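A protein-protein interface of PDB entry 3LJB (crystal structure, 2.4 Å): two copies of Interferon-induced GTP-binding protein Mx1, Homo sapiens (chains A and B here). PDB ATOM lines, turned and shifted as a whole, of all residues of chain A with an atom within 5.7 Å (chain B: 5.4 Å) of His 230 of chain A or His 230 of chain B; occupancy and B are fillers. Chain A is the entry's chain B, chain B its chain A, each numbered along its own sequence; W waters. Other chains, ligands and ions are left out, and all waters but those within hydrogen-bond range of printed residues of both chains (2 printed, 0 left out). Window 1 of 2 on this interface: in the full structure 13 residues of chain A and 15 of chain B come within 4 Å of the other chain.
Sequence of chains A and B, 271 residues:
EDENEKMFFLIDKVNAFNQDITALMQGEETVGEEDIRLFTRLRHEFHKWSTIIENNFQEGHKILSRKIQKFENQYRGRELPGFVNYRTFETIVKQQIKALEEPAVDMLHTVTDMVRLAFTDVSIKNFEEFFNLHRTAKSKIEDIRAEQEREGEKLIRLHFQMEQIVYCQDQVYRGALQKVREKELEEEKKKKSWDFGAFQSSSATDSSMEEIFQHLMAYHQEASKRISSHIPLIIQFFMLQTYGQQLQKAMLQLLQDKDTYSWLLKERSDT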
ATOM      1  N   HIS A 159       3.250  18.839 -12.701  1.00  0.00           N
ATOM      2  CA  HIS A 159       3.168  20.176 -13.289  1.00  0.00           C
ATOM      3  C   HIS A 159       3.445  20.180 -14.793  1.00  0.00           C
ATOM      4  O   HIS A 159       2.694  20.780 -15.565  1.00  0.00           O
ATOM      5  CB  HIS A 159       4.094  21.187 -12.610  1.00  0.00           C
ATOM      6  CG  HIS A 159       3.824  22.586 -13.049  1.00  0.00           C
ATOM      7  ND1 HIS A 159       2.776  23.329 -12.551  1.00  0.00           N
ATOM      8  CD2 HIS A 159       4.399  23.344 -14.007  1.00  0.00           C
ATOM      9  CE1 HIS A 159       2.740  24.502 -13.161  1.00  0.00           C
ATOM     10  NE2 HIS A 159       3.716  24.538 -14.048  1.00  0.00           N
ATOM     11  N   MET A 162       0.619  18.917 -16.569  1.00  0.00           N
ATOM     12  CA  MET A 162      -0.426  19.930 -16.629  1.00  0.00           C
ATOM     13  C   MET A 162      -0.134  20.939 -17.711  1.00  0.00           C
ATOM     14  O   MET A 162      -1.038  21.346 -18.436  1.00  0.00           O
ATOM     15  CB  MET A 162      -0.561  20.663 -15.298  1.00  0.00           C
ATOM     16  CG  MET A 162      -1.033  19.779 -14.163  1.00  0.00           C
ATOM     17  SD  MET A 162      -1.620  20.741 -12.766  1.00  0.00           S
ATOM     18  CE  MET A 162      -1.934  19.457 -11.549  1.00  0.00           C
ATOM     19  N   LYS A 225       6.557  31.404 -17.770  1.00  0.00           N
ATOM     20  CA  LYS A 225       6.338  32.151 -16.532  1.00  0.00           C
ATOM     21  C   LYS A 225       5.895  31.272 -15.346  1.00  0.00           C
ATOM     22  O   LYS A 225       6.397  31.450 -14.243  1.00  0.00           O
ATOM     23  CB  LYS A 225       5.331  33.287 -16.751  1.00  0.00           C
ATOM     24  CG  LYS A 225       5.166  34.168 -15.520  1.00  0.00           C
ATOM     25  CD  LYS A 225       4.202  35.349 -15.731  1.00  0.00           C
ATOM     26  CE  LYS A 225       3.645  35.850 -14.368  1.00  0.00           C
ATOM     27  NZ  LYS A 225       3.137  37.256 -14.409  1.00  0.00           N
ATOM     28  N   ARG A 226       4.960  30.345 -15.564  1.00  0.00           N
ATOM     29  CA  ARG A 226       4.531  29.428 -14.496  1.00  0.00           C
ATOM     30  C   ARG A 226       5.682  28.530 -14.051  1.00  0.00           C
ATOM     31  O   ARG A 226       5.950  28.396 -12.862  1.00  0.00           O
ATOM     32  CB  ARG A 226       3.346  28.566 -14.940  1.00  0.00           C
ATOM     33  CG  ARG A 226       2.025  29.320 -15.025  1.00  0.00           C
ATOM     34  CD  ARG A 226       0.888  28.501 -15.673  1.00  0.00           C
ATOM     35  NE  ARG A 226       1.136  28.231 -17.094  1.00  0.00           N
ATOM     36  CZ  ARG A 226       0.205  28.003 -18.020  1.00  0.00           C
ATOM     37  NH1 ARG A 226      -1.081  28.000 -17.713  1.00  0.00           N
ATOM     38  NH2 ARG A 226       0.563  27.776 -19.280  1.00  0.00           N
ATOM     39  N   ILE A 227       6.379  27.931 -15.008  1.00  0.00           N
ATOM     40  CA  ILE A 227       7.517  27.081 -14.700  1.00  0.00           C
ATOM     41  C   ILE A 227       8.575  27.843 -13.883  1.00  0.00           C
ATOM     42  O   ILE A 227       9.085  27.330 -12.881  1.00  0.00           O
ATOM     43  CB  ILE A 227       8.176  26.533 -15.979  1.00  0.00           C
ATOM     44  CG1 ILE A 227       7.195  25.655 -16.770  1.00  0.00           C
ATOM     45  CG2 ILE A 227       9.423  25.758 -15.651  1.00  0.00           C
ATOM     46  CD1 ILE A 227       6.538  24.596 -15.962  1.00  0.00           C
ATOM     47  N   SER A 228       8.879  29.070 -14.307  1.00  0.00           N
ATOM     48  CA  SER A 228       9.901  29.884 -13.662  1.00  0.00           C
ATOM     49  C   SER A 228       9.670  29.998 -12.180  1.00  0.00           C
ATOM     50  O   SER A 228      10.595  29.849 -11.399  1.00  0.00           O
ATOM     51  CB  SER A 228       9.953  31.286 -14.271  1.00  0.00           C
ATOM     52  OG  SER A 228      10.885  32.078 -13.564  1.00  0.00           O
ATOM     53  N   SER A 229       8.424  30.234 -11.790  1.00  0.00           N
ATOM     54  CA  SER A 229       8.085  30.403 -10.371  1.00  0.00           C
ATOM     55  C   SER A 229       7.704  29.120  -9.641  1.00  0.00           C
ATOM     56  O   SER A 229       8.100  28.937  -8.488  1.00  0.00           O
ATOM     57  CB  SER A 229       6.949  31.422 -10.211  1.00  0.00           C
ATOM     58  OG  SER A 229       6.025  31.320 -11.288  1.00  0.00           O
ATOM     59  N   HIS A 230       6.958  28.225 -10.285  1.00  0.00           N
ATOM     60  CA  HIS A 230       6.392  27.094  -9.552  1.00  0.00           C
ATOM     61  C   HIS A 230       7.415  26.018  -9.205  1.00  0.00           C
ATOM     62  O   HIS A 230       7.366  25.441  -8.109  1.00  0.00           O
ATOM     63  CB  HIS A 230       5.227  26.470 -10.303  1.00  0.00           C
ATOM     64  CG  HIS A 230       4.377  25.600  -9.440  1.00  0.00           C
ATOM     65  ND1 HIS A 230       3.700  26.084  -8.345  1.00  0.00           N
ATOM     66  CD2 HIS A 230       4.110  24.275  -9.490  1.00  0.00           C
ATOM     67  CE1 HIS A 230       3.039  25.098  -7.763  1.00  0.00           C
ATOM     68  NE2 HIS A 230       3.265  23.988  -8.441  1.00  0.00           N
ATOM     69  N   ILE A 231       8.345  25.740 -10.115  1.00  0.00           N
ATOM     70  CA  ILE A 231       9.350  24.715  -9.840  1.00  0.00           C
ATOM     71  C   ILE A 231      10.168  25.077  -8.590  1.00  0.00           C
ATOM     72  O   ILE A 231      10.245  24.250  -7.679  1.00  0.00           O
ATOM     73  CB  ILE A 231      10.246  24.355 -11.059  1.00  0.00           C
ATOM     74  CG1 ILE A 231       9.416  23.860 -12.254  1.00  0.00           C
ATOM     75  CG2 ILE A 231      11.182  23.262 -10.694  1.00  0.00           C
ATOM     76  CD1 ILE A 231       8.192  23.032 -11.906  1.00  0.00           C
ATOM     77  N   PRO A 232      10.720  26.315  -8.517  1.00  0.00           N
ATOM     78  CA  PRO A 232      11.365  26.712  -7.269  1.00  0.00           C
ATOM     79  C   PRO A 232      10.458  26.577  -6.050  1.00  0.00           C
ATOM     80  O   PRO A 232      10.884  26.080  -5.013  1.00  0.00           O
ATOM     81  CB  PRO A 232      11.758  28.170  -7.527  1.00  0.00           C
ATOM     82  CG  PRO A 232      12.108  28.173  -9.000  1.00  0.00           C
ATOM     83  CD  PRO A 232      11.012  27.291  -9.591  1.00  0.00           C
ATOM     84  N   LEU A 233       9.212  26.998  -6.179  1.00  0.00           N
ATOM     85  CA  LEU A 233       8.298  26.905  -5.049  1.00  0.00           C
ATOM     86  C   LEU A 233       8.179  25.435  -4.583  1.00  0.00           C
ATOM     87  O   LEU A 233       8.390  25.122  -3.390  1.00  0.00           O
ATOM     88  CB  LEU A 233       6.928  27.532  -5.392  1.00  0.00           C
ATOM     89  CG  LEU A 233       5.836  27.413  -4.314  1.00  0.00           C
ATOM     90  CD1 LEU A 233       6.093  28.381  -3.176  1.00  0.00           C
ATOM     91  CD2 LEU A 233       4.435  27.641  -4.885  1.00  0.00           C
ATOM     92  N   ILE A 234       7.875  24.527  -5.513  1.00  0.00           N
ATOM     93  CA  ILE A 234       7.784  23.098  -5.163  1.00  0.00           C
ATOM     94  C   ILE A 234       9.066  22.613  -4.451  1.00  0.00           C
ATOM     95  O   ILE A 234       9.021  21.928  -3.422  1.00  0.00           O
ATOM     96  CB  ILE A 234       7.532  22.217  -6.411  1.00  0.00           C
ATOM     97  CG1 ILE A 234       6.108  22.433  -6.948  1.00  0.00           C
ATOM     98  CG2 ILE A 234       7.803  20.729  -6.094  1.00  0.00           C
ATOM     99  CD1 ILE A 234       5.865  21.809  -8.358  1.00  0.00           C
ATOM    100  N   ILE A 235      10.209  23.000  -4.998  1.00  0.00           N
ATOM    101  CA  ILE A 235      11.496  22.523  -4.480  1.00  0.00           C
ATOM    102  C   ILE A 235      11.758  23.011  -3.042  1.00  0.00           C
ATOM    103  O   ILE A 235      12.183  22.243  -2.191  1.00  0.00           O
ATOM    104  CB  ILE A 235      12.627  22.913  -5.442  1.00  0.00           C
ATOM    105  CG1 ILE A 235      12.531  22.036  -6.697  1.00  0.00           C
ATOM    106  CG2 ILE A 235      13.976  22.777  -4.771  1.00  0.00           C
ATOM    107  CD1 ILE A 235      13.373  22.527  -7.807  1.00  0.00           C
ATOM    108  N   HIS B 159      -1.475  23.374  -2.711  1.00  0.00           N
ATOM    109  CA  HIS B 159      -0.926  24.591  -3.240  1.00  0.00           C
ATOM    110  C   HIS B 159      -0.987  25.647  -2.166  1.00  0.00           C
ATOM    111  O   HIS B 159      -0.022  26.380  -1.979  1.00  0.00           O
ATOM    112  CB  HIS B 159      -1.618  25.087  -4.507  1.00  0.00           C
ATOM    113  CG  HIS B 159      -0.932  26.272  -5.084  1.00  0.00           C
ATOM    114  ND1 HIS B 159       0.171  26.159  -5.903  1.00  0.00           N
ATOM    115  CD2 HIS B 159      -1.102  27.592  -4.857  1.00  0.00           C
ATOM    116  CE1 HIS B 159       0.615  27.366  -6.198  1.00  0.00           C
ATOM    117  NE2 HIS B 159      -0.137  28.253  -5.571  1.00  0.00           N
ATOM    118  N   MET B 162       1.661  25.366   0.365  1.00  0.00           N
ATOM    119  CA  MET B 162       2.944  25.809  -0.203  1.00  0.00           C
ATOM    120  C   MET B 162       3.060  27.308  -0.096  1.00  0.00           C
ATOM    121  O   MET B 162       4.145  27.821   0.125  1.00  0.00           O
ATOM    122  CB  MET B 162       3.122  25.412  -1.673  1.00  0.00           C
ATOM    123  CG  MET B 162       3.346  23.955  -1.879  1.00  0.00           C
ATOM    124  SD  MET B 162       3.912  23.483  -3.524  1.00  0.00           S
ATOM    125  CE  MET B 162       2.441  23.729  -4.515  1.00  0.00           C
ATOM    126  N   LYS B 225      -0.615  36.307  -7.870  1.00  0.00           N
ATOM    127  CA  LYS B 225      -0.454  35.940  -9.278  1.00  0.00           C
ATOM    128  C   LYS B 225      -0.476  34.431  -9.437  1.00  0.00           C
ATOM    129  O   LYS B 225      -1.156  33.909 -10.313  1.00  0.00           O
ATOM    130  CB  LYS B 225       0.854  36.496  -9.870  1.00  0.00           C
ATOM    131  CG  LYS B 225       0.980  38.034  -9.919  1.00  0.00           C
ATOM    132  CD  LYS B 225      -0.177  38.721 -10.646  1.00  0.00           C
ATOM    133  CE  LYS B 225      -0.001  40.256 -10.662  1.00  0.00           C
ATOM    134  NZ  LYS B 225      -1.251  40.984 -11.087  1.00  0.00           N
ATOM    135  N   ARG B 226       0.256  33.730  -8.583  1.00  0.00           N
ATOM    136  CA  ARG B 226       0.311  32.280  -8.668  1.00  0.00           C
ATOM    137  C   ARG B 226      -1.050  31.644  -8.414  1.00  0.00           C
ATOM    138  O   ARG B 226      -1.457  30.742  -9.133  1.00  0.00           O
ATOM    139  CB  ARG B 226       1.360  31.696  -7.712  1.00  0.00           C
ATOM    140  CG  ARG B 226       2.759  31.903  -8.200  1.00  0.00           C
ATOM    141  CD  ARG B 226       3.795  31.083  -7.424  1.00  0.00           C
ATOM    142  NE  ARG B 226       4.705  31.936  -6.647  1.00  0.00           N
ATOM    143  CZ  ARG B 226       4.488  32.335  -5.394  1.00  0.00           C
ATOM    144  NH1 ARG B 226       3.397  31.963  -4.749  1.00  0.00           N
ATOM    145  NH2 ARG B 226       5.369  33.106  -4.776  1.00  0.00           N
ATOM    146  N   ILE B 227      -1.765  32.112  -7.404  1.00  0.00           N
ATOM    147  CA  ILE B 227      -3.054  31.510  -7.082  1.00  0.00           C
ATOM    148  C   ILE B 227      -4.032  31.778  -8.217  1.00  0.00           C
ATOM    149  O   ILE B 227      -4.809  30.900  -8.572  1.00  0.00           O
ATOM    150  CB  ILE B 227      -3.604  32.018  -5.752  1.00  0.00           C
ATOM    151  CG1 ILE B 227      -2.712  31.552  -4.600  1.00  0.00           C
ATOM    152  CG2 ILE B 227      -5.014  31.514  -5.527  1.00  0.00           C
ATOM    153  CD1 ILE B 227      -2.824  32.442  -3.381  1.00  0.00           C
ATOM    154  N   SER B 228      -3.953  32.968  -8.812  1.00  0.00           N
ATOM    155  CA  SER B 228      -4.848  33.360  -9.910  1.00  0.00           C
ATOM    156  C   SER B 228      -4.664  32.488 -11.136  1.00  0.00           C
ATOM    157  O   SER B 228      -5.600  32.233 -11.895  1.00  0.00           O
ATOM    158  CB  SER B 228      -4.596  34.820 -10.304  1.00  0.00           C
ATOM    159  OG  SER B 228      -5.576  35.265 -11.223  1.00  0.00           O
ATOM    160  N   SER B 229      -3.446  32.010 -11.306  1.00  0.00           N
ATOM    161  CA  SER B 229      -3.093  31.267 -12.487  1.00  0.00           C
ATOM    162  C   SER B 229      -3.172  29.754 -12.254  1.00  0.00           C
ATOM    163  O   SER B 229      -3.770  29.033 -13.056  1.00  0.00           O
ATOM    164  CB  SER B 229      -1.702  31.689 -12.952  1.00  0.00           C
ATOM    165  OG  SER B 229      -1.252  30.814 -13.965  1.00  0.00           O
ATOM    166  N   HIS B 230      -2.626  29.285 -11.135  1.00  0.00           N
ATOM    167  CA  HIS B 230      -2.443  27.851 -10.920  1.00  0.00           C
ATOM    168  C   HIS B 230      -3.704  27.100 -10.489  1.00  0.00           C
ATOM    169  O   HIS B 230      -3.849  25.911 -10.793  1.00  0.00           O
ATOM    170  CB  HIS B 230      -1.340  27.590  -9.909  1.00  0.00           C
ATOM    171  CG  HIS B 230      -0.852  26.176  -9.920  1.00  0.00           C
ATOM    172  ND1 HIS B 230      -0.361  25.577 -11.057  1.00  0.00           N
ATOM    173  CD2 HIS B 230      -0.778  25.244  -8.941  1.00  0.00           C
ATOM    174  CE1 HIS B 230      -0.013  24.334 -10.782  1.00  0.00           C
ATOM    175  NE2 HIS B 230      -0.251  24.109  -9.502  1.00  0.00           N
ATOM    176  N   ILE B 231      -4.618  27.764  -9.789  1.00  0.00           N
ATOM    177  CA  ILE B 231      -5.854  27.075  -9.386  1.00  0.00           C
ATOM    178  C   ILE B 231      -6.750  26.722 -10.605  1.00  0.00           C
ATOM    179  O   ILE B 231      -7.233  25.594 -10.704  1.00  0.00           O
ATOM    180  CB  ILE B 231      -6.684  27.828  -8.287  1.00  0.00           C
ATOM    181  CG1 ILE B 231      -5.860  28.094  -7.014  1.00  0.00           C
ATOM    182  CG2 ILE B 231      -7.932  27.025  -7.947  1.00  0.00           C
ATOM    183  CD1 ILE B 231      -4.905  26.978  -6.583  1.00  0.00           C
ATOM    184  N   PRO B 232      -6.978  27.676 -11.534  1.00  0.00           N
ATOM    185  CA  PRO B 232      -7.716  27.309 -12.755  1.00  0.00           C
ATOM    186  C   PRO B 232      -7.017  26.235 -13.597  1.00  0.00           C
ATOM    187  O   PRO B 232      -7.674  25.389 -14.200  1.00  0.00           O
ATOM    188  CB  PRO B 232      -7.787  28.626 -13.523  1.00  0.00           C
ATOM    189  CG  PRO B 232      -7.805  29.652 -12.484  1.00  0.00           C
ATOM    190  CD  PRO B 232      -6.924  29.138 -11.362  1.00  0.00           C
ATOM    191  N   LEU B 233      -5.693  26.274 -13.635  1.00  0.00           N
ATOM    192  CA  LEU B 233      -4.920  25.235 -14.296  1.00  0.00           C
ATOM    193  C   LEU B 233      -5.180  23.866 -13.663  1.00  0.00           C
ATOM    194  O   LEU B 233      -5.391  22.879 -14.360  1.00  0.00           O
ATOM    195  CB  LEU B 233      -3.435  25.575 -14.219  1.00  0.00           C
ATOM    196  CG  LEU B 233      -2.490  24.613 -14.923  1.00  0.00           C
ATOM    197  CD1 LEU B 233      -2.877  24.500 -16.394  1.00  0.00           C
ATOM    198  CD2 LEU B 233      -1.062  25.059 -14.756  1.00  0.00           C
ATOM    199  N   ILE B 234      -5.163  23.805 -12.339  1.00  0.00           N
ATOM    200  CA  ILE B 234      -5.436  22.552 -11.631  1.00  0.00           C
ATOM    201  C   ILE B 234      -6.840  22.075 -11.963  1.00  0.00           C
ATOM    202  O   ILE B 234      -7.046  20.931 -12.337  1.00  0.00           O
ATOM    203  CB  ILE B 234      -5.257  22.714 -10.085  1.00  0.00           C
ATOM    204  CG1 ILE B 234      -3.765  22.847  -9.737  1.00  0.00           C
ATOM    205  CG2 ILE B 234      -5.890  21.528  -9.319  1.00  0.00           C
ATOM    206  CD1 ILE B 234      -3.516  23.434  -8.326  1.00  0.00           C
ATOM    207  N   ILE B 235      -7.803  22.968 -11.835  1.00  0.00           N
ATOM    208  CA  ILE B 235      -9.205  22.629 -12.071  1.00  0.00           C
ATOM    209  C   ILE B 235      -9.471  22.105 -13.512  1.00  0.00           C
ATOM    210  O   ILE B 235     -10.114  21.088 -13.728  1.00  0.00           O
ATOM    211  CB  ILE B 235     -10.068  23.861 -11.757  1.00  0.00           C
ATOM    212  CG1 ILE B 235     -10.112  24.073 -10.232  1.00  0.00           C
ATOM    213  CG2 ILE B 235     -11.487  23.708 -12.320  1.00  0.00           C
ATOM    214  CD1 ILE B 235     -10.657  25.423  -9.799  1.00  0.00           C
HETATM  215  O   HOH W   1       2.100  22.442 -10.071  1.00  0.00           O
HETATM  216  O   HOH W   2       0.406  23.514  -6.710  1.00  0.00           O
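O of Arg 226 of chain A is in hydrogen-bond range of OG of Ser 229 of chain A (3.3 Å).
His 159 of chain A touches His 230 of chain B, and with the chains exchanged His 230 of chain A touches His 159 of chain B.
Arg 226 of chain A touches Ser 229 of chain B, but with the chains exchanged Ser 229 of chain A does not touch Arg 226 of chain B (4.2 Å).
His 230 of chain A touches Met 162 of chain B, but with the chains exchanged Met 162 of chain A does not touch His 230 of chain B (4.4 Å).
Leu 233 of chain A touches Met 162 of chain B, but with the chains exchanged Met 162 of chain A does not touch Leu 233 of chain B (4.2 Å).
Printed residues of chain B within 4 Å of His 159 of chain A: His 230 (3.5 Å).
Of the printed residues of chain B, His 230 of chain A touches His 159, Met 162 and His 230.
Of the printed residues of chain B, Leu 233 of chain A touches Met 162 (3.9 Å).
Of the printed residues of chain A, Met 162 of chain B touches His 230 (3.6 Å) and Leu 233 (3.9 Å).
Of the printed residues of chain A, Ser 229 of chain B touches Arg 226.
Of the printed residues of chain A, His 230 of chain B touches His 159 and His 230.
Leu 233 of chain B touches none of the printed residues of chain A.
The nearest printed residue of chain A that does not touch His 230 of chain B is Met 162 of chain A (4.4 Å).
The nearest printed residue of chain A that does not touch Ser 229 of chain B is Lys 225 of chain A (6.9 Å).
Water W1 lies within hydrogen-bond range of NE2 of His 230 of chain A (2.5 Å), ND1 of His 159 of chain A (2.7 Å) and NE2 of His 230 of chain B (2.9 Å).
Water W2 lies within hydrogen-bond range of ND1 of His 159 of chain B, NE2 of His 230 of chain B and NE2 of His 230 of chain A.
His 230 of chain B touches His 159 of chain A (CE1 to ND1, 3.5 Å).
Arg 226 of chain A touches Ser 229 of chain B.
His 230 of chain A touches His 159 of chain B.
Met 162 of chain B touches His 230 of chain A (CE to CE1, 3.6 Å).
NE2 of His 230 of chain A touches NE2 of His 230 of chain B, at 3.7 Å.
Leu 233 of chain A touches Met 162 of chain B.
Hydrophobic or aromatic side chains of chain B that line the printed part of chain A: His 159, Met 162 and His 230.
Along chain B the printed residues that touch a printed residue of chain A span positions 159 to 230.
Among the printed residues, no Asp or Glu carboxylate lies within 4 Å of a Lys or Arg side-chain nitrogen of the other chain.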
